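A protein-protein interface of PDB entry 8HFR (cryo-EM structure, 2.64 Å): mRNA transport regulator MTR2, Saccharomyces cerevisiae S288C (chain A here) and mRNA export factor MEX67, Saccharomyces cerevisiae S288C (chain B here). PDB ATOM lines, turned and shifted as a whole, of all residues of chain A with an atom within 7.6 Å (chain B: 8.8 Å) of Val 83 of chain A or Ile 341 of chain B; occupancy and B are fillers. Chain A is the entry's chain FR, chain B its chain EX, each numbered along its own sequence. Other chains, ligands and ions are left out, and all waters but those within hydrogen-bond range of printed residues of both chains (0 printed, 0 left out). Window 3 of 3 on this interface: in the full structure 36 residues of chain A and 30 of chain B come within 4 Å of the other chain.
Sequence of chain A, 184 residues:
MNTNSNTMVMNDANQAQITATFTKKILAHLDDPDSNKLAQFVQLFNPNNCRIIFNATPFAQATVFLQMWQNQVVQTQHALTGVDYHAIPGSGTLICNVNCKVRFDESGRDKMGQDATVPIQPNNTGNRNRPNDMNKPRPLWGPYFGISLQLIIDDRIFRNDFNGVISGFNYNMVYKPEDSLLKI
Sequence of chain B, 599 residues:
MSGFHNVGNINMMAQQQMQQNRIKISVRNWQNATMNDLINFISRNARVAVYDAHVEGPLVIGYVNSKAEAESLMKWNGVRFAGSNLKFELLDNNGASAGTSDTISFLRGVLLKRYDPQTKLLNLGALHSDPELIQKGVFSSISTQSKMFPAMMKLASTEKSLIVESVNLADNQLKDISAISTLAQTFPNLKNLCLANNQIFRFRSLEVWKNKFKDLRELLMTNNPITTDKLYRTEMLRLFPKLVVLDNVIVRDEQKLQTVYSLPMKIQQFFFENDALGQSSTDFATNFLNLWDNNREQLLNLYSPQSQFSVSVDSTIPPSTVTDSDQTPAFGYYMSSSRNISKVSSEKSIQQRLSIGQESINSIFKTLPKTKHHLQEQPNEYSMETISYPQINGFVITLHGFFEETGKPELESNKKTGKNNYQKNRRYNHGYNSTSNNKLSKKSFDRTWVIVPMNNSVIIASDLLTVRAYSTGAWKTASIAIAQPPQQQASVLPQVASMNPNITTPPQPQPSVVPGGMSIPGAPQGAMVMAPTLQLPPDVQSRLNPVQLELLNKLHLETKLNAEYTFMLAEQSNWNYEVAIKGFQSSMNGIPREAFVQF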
ATOM      1  N   ALA A  13      12.430  -2.366 -23.035  1.00  0.00           N
ATOM      2  CA  ALA A  13      12.973  -2.110 -21.704  1.00  0.00           C
ATOM      3  C   ALA A  13      11.996  -2.379 -20.565  1.00  0.00           C
ATOM      4  O   ALA A  13      12.447  -2.571 -19.425  1.00  0.00           O
ATOM      5  CB  ALA A  13      13.471  -0.662 -21.594  1.00  0.00           C
ATOM      6  N   ALA A  16      12.847  -5.783 -19.482  1.00  0.00           N
ATOM      7  CA  ALA A  16      14.057  -5.796 -18.669  1.00  0.00           C
ATOM      8  C   ALA A  16      13.773  -5.341 -17.245  1.00  0.00           C
ATOM      9  O   ALA A  16      14.272  -5.943 -16.286  1.00  0.00           O
ATOM     10  CB  ALA A  16      15.123  -4.917 -19.322  1.00  0.00           C
ATOM     11  N   GLN A  17      12.931  -4.313 -17.089  1.00  0.00           N
ATOM     12  CA  GLN A  17      12.575  -3.827 -15.756  1.00  0.00           C
ATOM     13  C   GLN A  17      11.759  -4.856 -14.971  1.00  0.00           C
ATOM     14  O   GLN A  17      12.017  -5.080 -13.779  1.00  0.00           O
ATOM     15  CB  GLN A  17      11.810  -2.509 -15.865  1.00  0.00           C
ATOM     16  N   THR A  19      11.733  -8.147 -15.461  1.00  0.00           N
ATOM     17  CA  THR A  19      12.612  -9.267 -15.156  1.00  0.00           C
ATOM     18  C   THR A  19      13.567  -8.928 -14.020  1.00  0.00           C
ATOM     19  O   THR A  19      13.829  -9.775 -13.162  1.00  0.00           O
ATOM     20  CB  THR A  19      13.386  -9.682 -16.407  1.00  0.00           C
ATOM     21  N   ALA A  20      14.059  -7.681 -13.969  1.00  0.00           N
ATOM     22  CA  ALA A  20      14.949  -7.278 -12.881  1.00  0.00           C
ATOM     23  C   ALA A  20      14.213  -7.232 -11.548  1.00  0.00           C
ATOM     24  O   ALA A  20      14.773  -7.614 -10.512  1.00  0.00           O
ATOM     25  CB  ALA A  20      15.579  -5.921 -13.193  1.00  0.00           C
ATOM     26  N   THR A  21      12.946  -6.801 -11.566  1.00  0.00           N
ATOM     27  CA  THR A  21      12.139  -6.773 -10.345  1.00  0.00           C
ATOM     28  C   THR A  21      11.901  -8.177  -9.810  1.00  0.00           C
ATOM     29  O   THR A  21      12.122  -8.450  -8.617  1.00  0.00           O
ATOM     30  CB  THR A  21      10.809  -6.069 -10.616  1.00  0.00           C
ATOM     31  N   THR A  23      13.678 -10.813 -10.525  1.00  0.00           N
ATOM     32  CA  THR A  23      14.960 -11.420 -10.199  1.00  0.00           C
ATOM     33  C   THR A  23      15.469 -10.960  -8.839  1.00  0.00           C
ATOM     34  O   THR A  23      16.007 -11.768  -8.076  1.00  0.00           O
ATOM     35  CB  THR A  23      15.978 -11.096 -11.294  1.00  0.00           C
ATOM     36  N   LEU A  80      22.732  -8.131  -6.115  1.00  0.00           N
ATOM     37  CA  LEU A  80      22.941  -8.144  -7.554  1.00  0.00           C
ATOM     38  C   LEU A  80      24.010  -7.132  -7.949  1.00  0.00           C
ATOM     39  O   LEU A  80      24.260  -6.155  -7.236  1.00  0.00           O
ATOM     40  CB  LEU A  80      21.641  -7.838  -8.299  1.00  0.00           C
ATOM     41  N   THR A  81      24.647  -7.377  -9.093  1.00  0.00           N
ATOM     42  CA  THR A  81      25.614  -6.443  -9.653  1.00  0.00           C
ATOM     43  C   THR A  81      25.200  -5.937 -11.023  1.00  0.00           C
ATOM     44  O   THR A  81      25.292  -4.733 -11.288  1.00  0.00           O
ATOM     45  CB  THR A  81      26.999  -7.106  -9.731  1.00  0.00           C
ATOM     46  N   GLY A  82      24.757  -6.831 -11.905  1.00  0.00           N
ATOM     47  CA  GLY A  82      24.283  -6.490 -13.240  1.00  0.00           C
ATOM     48  C   GLY A  82      23.435  -7.649 -13.736  1.00  0.00           C
ATOM     49  O   GLY A  82      23.478  -8.750 -13.178  1.00  0.00           O
ATOM     50  N   VAL A  83      22.666  -7.391 -14.795  1.00  0.00           N
ATOM     51  CA  VAL A  83      21.804  -8.404 -15.390  1.00  0.00           C
ATOM     52  C   VAL A  83      21.439  -7.983 -16.805  1.00  0.00           C
ATOM     53  O   VAL A  83      21.016  -6.843 -17.022  1.00  0.00           O
ATOM     54  CB  VAL A  83      20.530  -8.614 -14.560  1.00  0.00           C
ATOM     55  N   ASP A  84      21.591  -8.903 -17.758  1.00  0.00           N
ATOM     56  CA  ASP A  84      21.175  -8.676 -19.138  1.00  0.00           C
ATOM     57  C   ASP A  84      20.307  -9.839 -19.603  1.00  0.00           C
ATOM     58  O   ASP A  84      20.184 -10.854 -18.918  1.00  0.00           O
ATOM     59  CB  ASP A  84      22.376  -8.495 -20.075  1.00  0.00           C
ATOM     60  N   TYR A  85      19.703  -9.688 -20.782  1.00  0.00           N
ATOM     61  CA  TYR A  85      18.759 -10.675 -21.289  1.00  0.00           C
ATOM     62  C   TYR A  85      18.971 -10.906 -22.781  1.00  0.00           C
ATOM     63  O   TYR A  85      19.645 -10.133 -23.466  1.00  0.00           O
ATOM     64  CB  TYR A  85      17.307 -10.244 -21.030  1.00  0.00           C
ATOM     65  N   CYS A  96      18.103 -14.764 -19.492  1.00  0.00           N
ATOM     66  CA  CYS A  96      18.802 -13.689 -18.815  1.00  0.00           C
ATOM     67  C   CYS A  96      20.025 -14.257 -18.116  1.00  0.00           C
ATOM     68  O   CYS A  96      20.121 -15.458 -17.864  1.00  0.00           O
ATOM     69  CB  CYS A  96      17.889 -12.982 -17.805  1.00  0.00           C
ATOM     70  N   ASN A  97      20.970 -13.373 -17.819  1.00  0.00           N
ATOM     71  CA  ASN A  97      22.152 -13.720 -17.047  1.00  0.00           C
ATOM     72  C   ASN A  97      22.465 -12.567 -16.113  1.00  0.00           C
ATOM     73  O   ASN A  97      22.563 -11.416 -16.552  1.00  0.00           O
ATOM     74  CB  ASN A  97      23.352 -14.026 -17.951  1.00  0.00           C
ATOM     75  N   VAL A  98      22.604 -12.883 -14.826  1.00  0.00           N
ATOM     76  CA  VAL A  98      22.843 -11.902 -13.784  1.00  0.00           C
ATOM     77  C   VAL A  98      24.092 -12.276 -13.000  1.00  0.00           C
ATOM     78  O   VAL A  98      24.480 -13.447 -12.927  1.00  0.00           O
ATOM     79  CB  VAL A  98      21.641 -11.793 -12.833  1.00  0.00           C
ATOM     80  N   ASN A  99      24.729 -11.259 -12.431  1.00  0.00           N
ATOM     81  CA  ASN A  99      25.916 -11.423 -11.601  1.00  0.00           C
ATOM     82  C   ASN A  99      25.543 -11.183 -10.142  1.00  0.00           C
ATOM     83  O   ASN A  99      24.897 -10.178  -9.818  1.00  0.00           O
ATOM     84  CB  ASN A  99      27.024 -10.464 -12.043  1.00  0.00           C
ATOM     85  N   LEU A 149      24.699 -16.348 -12.666  1.00  0.00           N
ATOM     86  CA  LEU A 149      23.558 -17.242 -12.815  1.00  0.00           C
ATOM     87  C   LEU A 149      22.780 -16.858 -14.066  1.00  0.00           C
ATOM     88  O   LEU A 149      22.364 -15.706 -14.217  1.00  0.00           O
ATOM     89  CB  LEU A 149      22.651 -17.198 -11.582  1.00  0.00           C
ATOM     90  N   SER B 310      23.682 -10.087 -26.394  1.00  0.00           N
ATOM     91  CA  SER B 310      23.648  -9.134 -25.289  1.00  0.00           C
ATOM     92  C   SER B 310      25.078  -8.708 -24.986  1.00  0.00           C
ATOM     93  O   SER B 310      26.036  -9.191 -25.595  1.00  0.00           O
ATOM     94  CB  SER B 310      22.968  -9.727 -24.049  1.00  0.00           C
ATOM     95  N   VAL B 311      25.210  -7.781 -24.034  1.00  0.00           N
ATOM     96  CA  VAL B 311      26.526  -7.336 -23.578  1.00  0.00           C
ATOM     97  C   VAL B 311      26.353  -6.815 -22.152  1.00  0.00           C
ATOM     98  O   VAL B 311      25.926  -5.674 -21.958  1.00  0.00           O
ATOM     99  CB  VAL B 311      27.102  -6.269 -24.494  1.00  0.00           C
ATOM    100  N   SER B 312      26.696  -7.647 -21.172  1.00  0.00           N
ATOM    101  CA  SER B 312      26.586  -7.289 -19.767  1.00  0.00           C
ATOM    102  C   SER B 312      27.962  -6.991 -19.196  1.00  0.00           C
ATOM    103  O   SER B 312      28.940  -7.674 -19.516  1.00  0.00           O
ATOM    104  CB  SER B 312      25.922  -8.402 -18.956  1.00  0.00           C
ATOM    105  N   VAL B 313      28.028  -5.973 -18.343  1.00  0.00           N
ATOM    106  CA  VAL B 313      29.262  -5.571 -17.684  1.00  0.00           C
ATOM    107  C   VAL B 313      28.978  -5.371 -16.205  1.00  0.00           C
ATOM    108  O   VAL B 313      28.170  -4.512 -15.838  1.00  0.00           O
ATOM    109  CB  VAL B 313      29.837  -4.294 -18.304  1.00  0.00           C
ATOM    110  N   ASP B 314      29.639  -6.164 -15.363  1.00  0.00           N
ATOM    111  CA  ASP B 314      29.532  -6.033 -13.913  1.00  0.00           C
ATOM    112  C   ASP B 314      30.546  -4.997 -13.444  1.00  0.00           C
ATOM    113  O   ASP B 314      31.752  -5.264 -13.419  1.00  0.00           O
ATOM    114  CB  ASP B 314      29.764  -7.378 -13.231  1.00  0.00           C
ATOM    115  N   SER B 315      30.055  -3.816 -13.060  1.00  0.00           N
ATOM    116  CA  SER B 315      30.921  -2.697 -12.705  1.00  0.00           C
ATOM    117  C   SER B 315      31.531  -2.826 -11.315  1.00  0.00           C
ATOM    118  O   SER B 315      32.389  -2.012 -10.961  1.00  0.00           O
ATOM    119  CB  SER B 315      30.142  -1.388 -12.808  1.00  0.00           C
ATOM    120  N   SER B 338      27.466  -0.408 -23.493  1.00  0.00           N
ATOM    121  CA  SER B 338      26.953  -0.913 -22.225  1.00  0.00           C
ATOM    122  C   SER B 338      25.439  -1.089 -22.262  1.00  0.00           C
ATOM    123  O   SER B 338      24.707  -0.238 -22.775  1.00  0.00           O
ATOM    124  CB  SER B 338      27.335   0.034 -21.089  1.00  0.00           C
ATOM    125  N   ARG B 339      24.978  -2.211 -21.699  1.00  0.00           N
ATOM    126  CA  ARG B 339      23.547  -2.480 -21.560  1.00  0.00           C
ATOM    127  C   ARG B 339      23.373  -3.452 -20.390  1.00  0.00           C
ATOM    128  O   ARG B 339      23.628  -4.650 -20.538  1.00  0.00           O
ATOM    129  CB  ARG B 339      22.965  -3.040 -22.849  1.00  0.00           C
ATOM    130  N   ASN B 340      22.939  -2.927 -19.244  1.00  0.00           N
ATOM    131  CA  ASN B 340      22.697  -3.749 -18.061  1.00  0.00           C
ATOM    132  C   ASN B 340      21.702  -3.024 -17.170  1.00  0.00           C
ATOM    133  O   ASN B 340      21.884  -1.837 -16.882  1.00  0.00           O
ATOM    134  CB  ASN B 340      23.996  -4.028 -17.293  1.00  0.00           C
ATOM    135  N   ILE B 341      20.675  -3.748 -16.715  1.00  0.00           N
ATOM    136  CA  ILE B 341      19.527  -3.111 -16.070  1.00  0.00           C
ATOM    137  C   ILE B 341      19.861  -2.562 -14.688  1.00  0.00           C
ATOM    138  O   ILE B 341      19.123  -1.719 -14.165  1.00  0.00           O
ATOM    139  CB  ILE B 341      18.363  -4.099 -15.976  1.00  0.00           C
ATOM    140  N   SER B 342      20.958  -3.019 -14.079  1.00  0.00           N
ATOM    141  CA  SER B 342      21.342  -2.498 -12.770  1.00  0.00           C
ATOM    142  C   SER B 342      21.908  -1.088 -12.881  1.00  0.00           C
ATOM    143  O   SER B 342      21.763  -0.282 -11.955  1.00  0.00           O
ATOM    144  CB  SER B 342      22.347  -3.433 -12.105  1.00  0.00           C
ATOM    145  N   LYS B 343      22.546  -0.768 -14.006  1.00  0.00           N
ATOM    146  CA  LYS B 343      23.096   0.561 -14.234  1.00  0.00           C
ATOM    147  C   LYS B 343      22.238   1.424 -15.144  1.00  0.00           C
ATOM    148  O   LYS B 343      22.210   2.647 -14.968  1.00  0.00           O
ATOM    149  CB  LYS B 343      24.507   0.457 -14.825  1.00  0.00           C
ATOM    150  N   VAL B 344      21.529   0.826 -16.100  1.00  0.00           N
ATOM    151  CA  VAL B 344      20.770   1.601 -17.072  1.00  0.00           C
ATOM    152  C   VAL B 344      19.446   2.085 -16.488  1.00  0.00           C
ATOM    153  O   VAL B 344      18.872   1.470 -15.585  1.00  0.00           O
ATOM    154  CB  VAL B 344      20.510   0.772 -18.328  1.00  0.00           C
ATOM    155  N   SER B 345      18.972   3.225 -17.005  1.00  0.00           N
ATOM    156  CA  SER B 345      17.645   3.726 -16.668  1.00  0.00           C
ATOM    157  C   SER B 345      16.895   4.349 -17.842  1.00  0.00           C
ATOM    158  O   SER B 345      15.753   4.781 -17.653  1.00  0.00           O
ATOM    159  CB  SER B 345      17.737   4.746 -15.525  1.00  0.00           C
ATOM    160  N   SER B 346      17.487   4.416 -19.034  1.00  0.00           N
ATOM    161  CA  SER B 346      16.885   5.067 -20.194  1.00  0.00           C
ATOM    162  C   SER B 346      16.288   4.007 -21.105  1.00  0.00           C
ATOM    163  O   SER B 346      17.018   3.168 -21.642  1.00  0.00           O
ATOM    164  CB  SER B 346      17.917   5.898 -20.957  1.00  0.00           C
ATOM    165  N   ILE B 350      18.067   1.996 -24.040  1.00  0.00           N
ATOM    166  CA  ILE B 350      18.169   0.564 -23.774  1.00  0.00           C
ATOM    167  C   ILE B 350      17.576  -0.258 -24.914  1.00  0.00           C
ATOM    168  O   ILE B 350      18.049  -1.363 -25.202  1.00  0.00           O
ATOM    169  CB  ILE B 350      17.480   0.228 -22.450  1.00  0.00           C
ATOM    170  N   LEU B 465      27.176 -12.270 -23.899  1.00  0.00           N
ATOM    171  CA  LEU B 465      28.492 -12.111 -23.284  1.00  0.00           C
ATOM    172  C   LEU B 465      28.342 -11.246 -22.045  1.00  0.00           C
ATOM    173  O   LEU B 465      27.921 -10.088 -22.149  1.00  0.00           O
ATOM    174  CB  LEU B 465      29.490 -11.483 -24.263  1.00  0.00           C
ATOM    175  N   THR B 466      28.681 -11.800 -20.883  1.00  0.00           N
ATOM    176  CA  THR B 466      28.668 -11.073 -19.619  1.00  0.00           C
ATOM    177  C   THR B 466      30.067 -11.097 -19.024  1.00  0.00           C
ATOM    178  O   THR B 466      30.627 -12.172 -18.801  1.00  0.00           O
ATOM    179  CB  THR B 466      27.658 -11.679 -18.641  1.00  0.00           C
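Among the printed residues, pairs that only touch across the chains: Thr 81 of chain A with Ser 342 of chain B (3.3 Å), Gly 82 of chain A with Ser 342 of chain B (3.8 Å), Val 83 of chain A with Asn 340 of chain B (3.7 Å), Asp 84 of chain A with Ser 312 of chain B (3.7 Å) and Tyr 85 of chain A with Ser 310 of chain B (3.4 Å).
Printed residues of chain B that touch a printed residue of chain A: Ser 310, Ser 312, Asn 340, Ile 341 and Ser 342.
Hydrophobic or aromatic side chains of chain B within 4 Å of the printed part of chain A: Ile 341.
Of the 18 printed residues of chain A, 5 touch a printed residue of chain B.
Printed residues of chain A that touch a printed residue of chain B: Thr 81, Gly 82, Val 83, Asp 84 and Tyr 85.
Among the printed residues, 6 pairs touch across the chains.
Among the printed residues, no Asp or Glu carboxylate lies within 4 Å of a Lys or Arg side-chain nitrogen of the other chain.
Of the printed residues of chain B, Thr 81 of chain A touches Ser 342.
Gly 82 of chain A touches just one residue of chain B: Ser 342 (3.8 Å).
Val 83 of chain A touches just these residues of chain B: Asn 340 and Ile 341.
Asp 84 of chain A touches one residue of chain B.
Of the printed residues of chain B, Tyr 85 of chain A touches Ser 310.
Printed residues of chain A within 4 Å of Ser 310 of chain B: Tyr 85 (3.4 Å).
Of chain A, only Val 83 comes within 4 Å of Ile 341 of chain B.
The nearest residue of chain A that does not touch Ile 341 of chain B is Ala 20 of chain A (4.3 Å).
The backbone carbonyl oxygen of Val 83 of chain A is in hydrogen-bond range of the backbone NH of Ile 341 of chain B, 3.1 Å away.
N of Asn 99 of chain A is in hydrogen-bond range of O of Gly 82 of chain A, 2.9 Å away.
The backbone NH (N) of Ser 312 of chain B lies within hydrogen-bond range of the backbone carbonyl oxygen (O) of Leu 465 of chain B, at 2.9 Å.
The backbone NH of Thr 81 of chain A lies within hydrogen-bond range of the backbone carbonyl oxygen of Asn 99 of chain A, at 2.9 Å.
The backbone carbonyl oxygen of Asp 84 of chain A sits at hydrogen-bond distance from the backbone NH of Asn 97 of chain A (2.9 Å).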
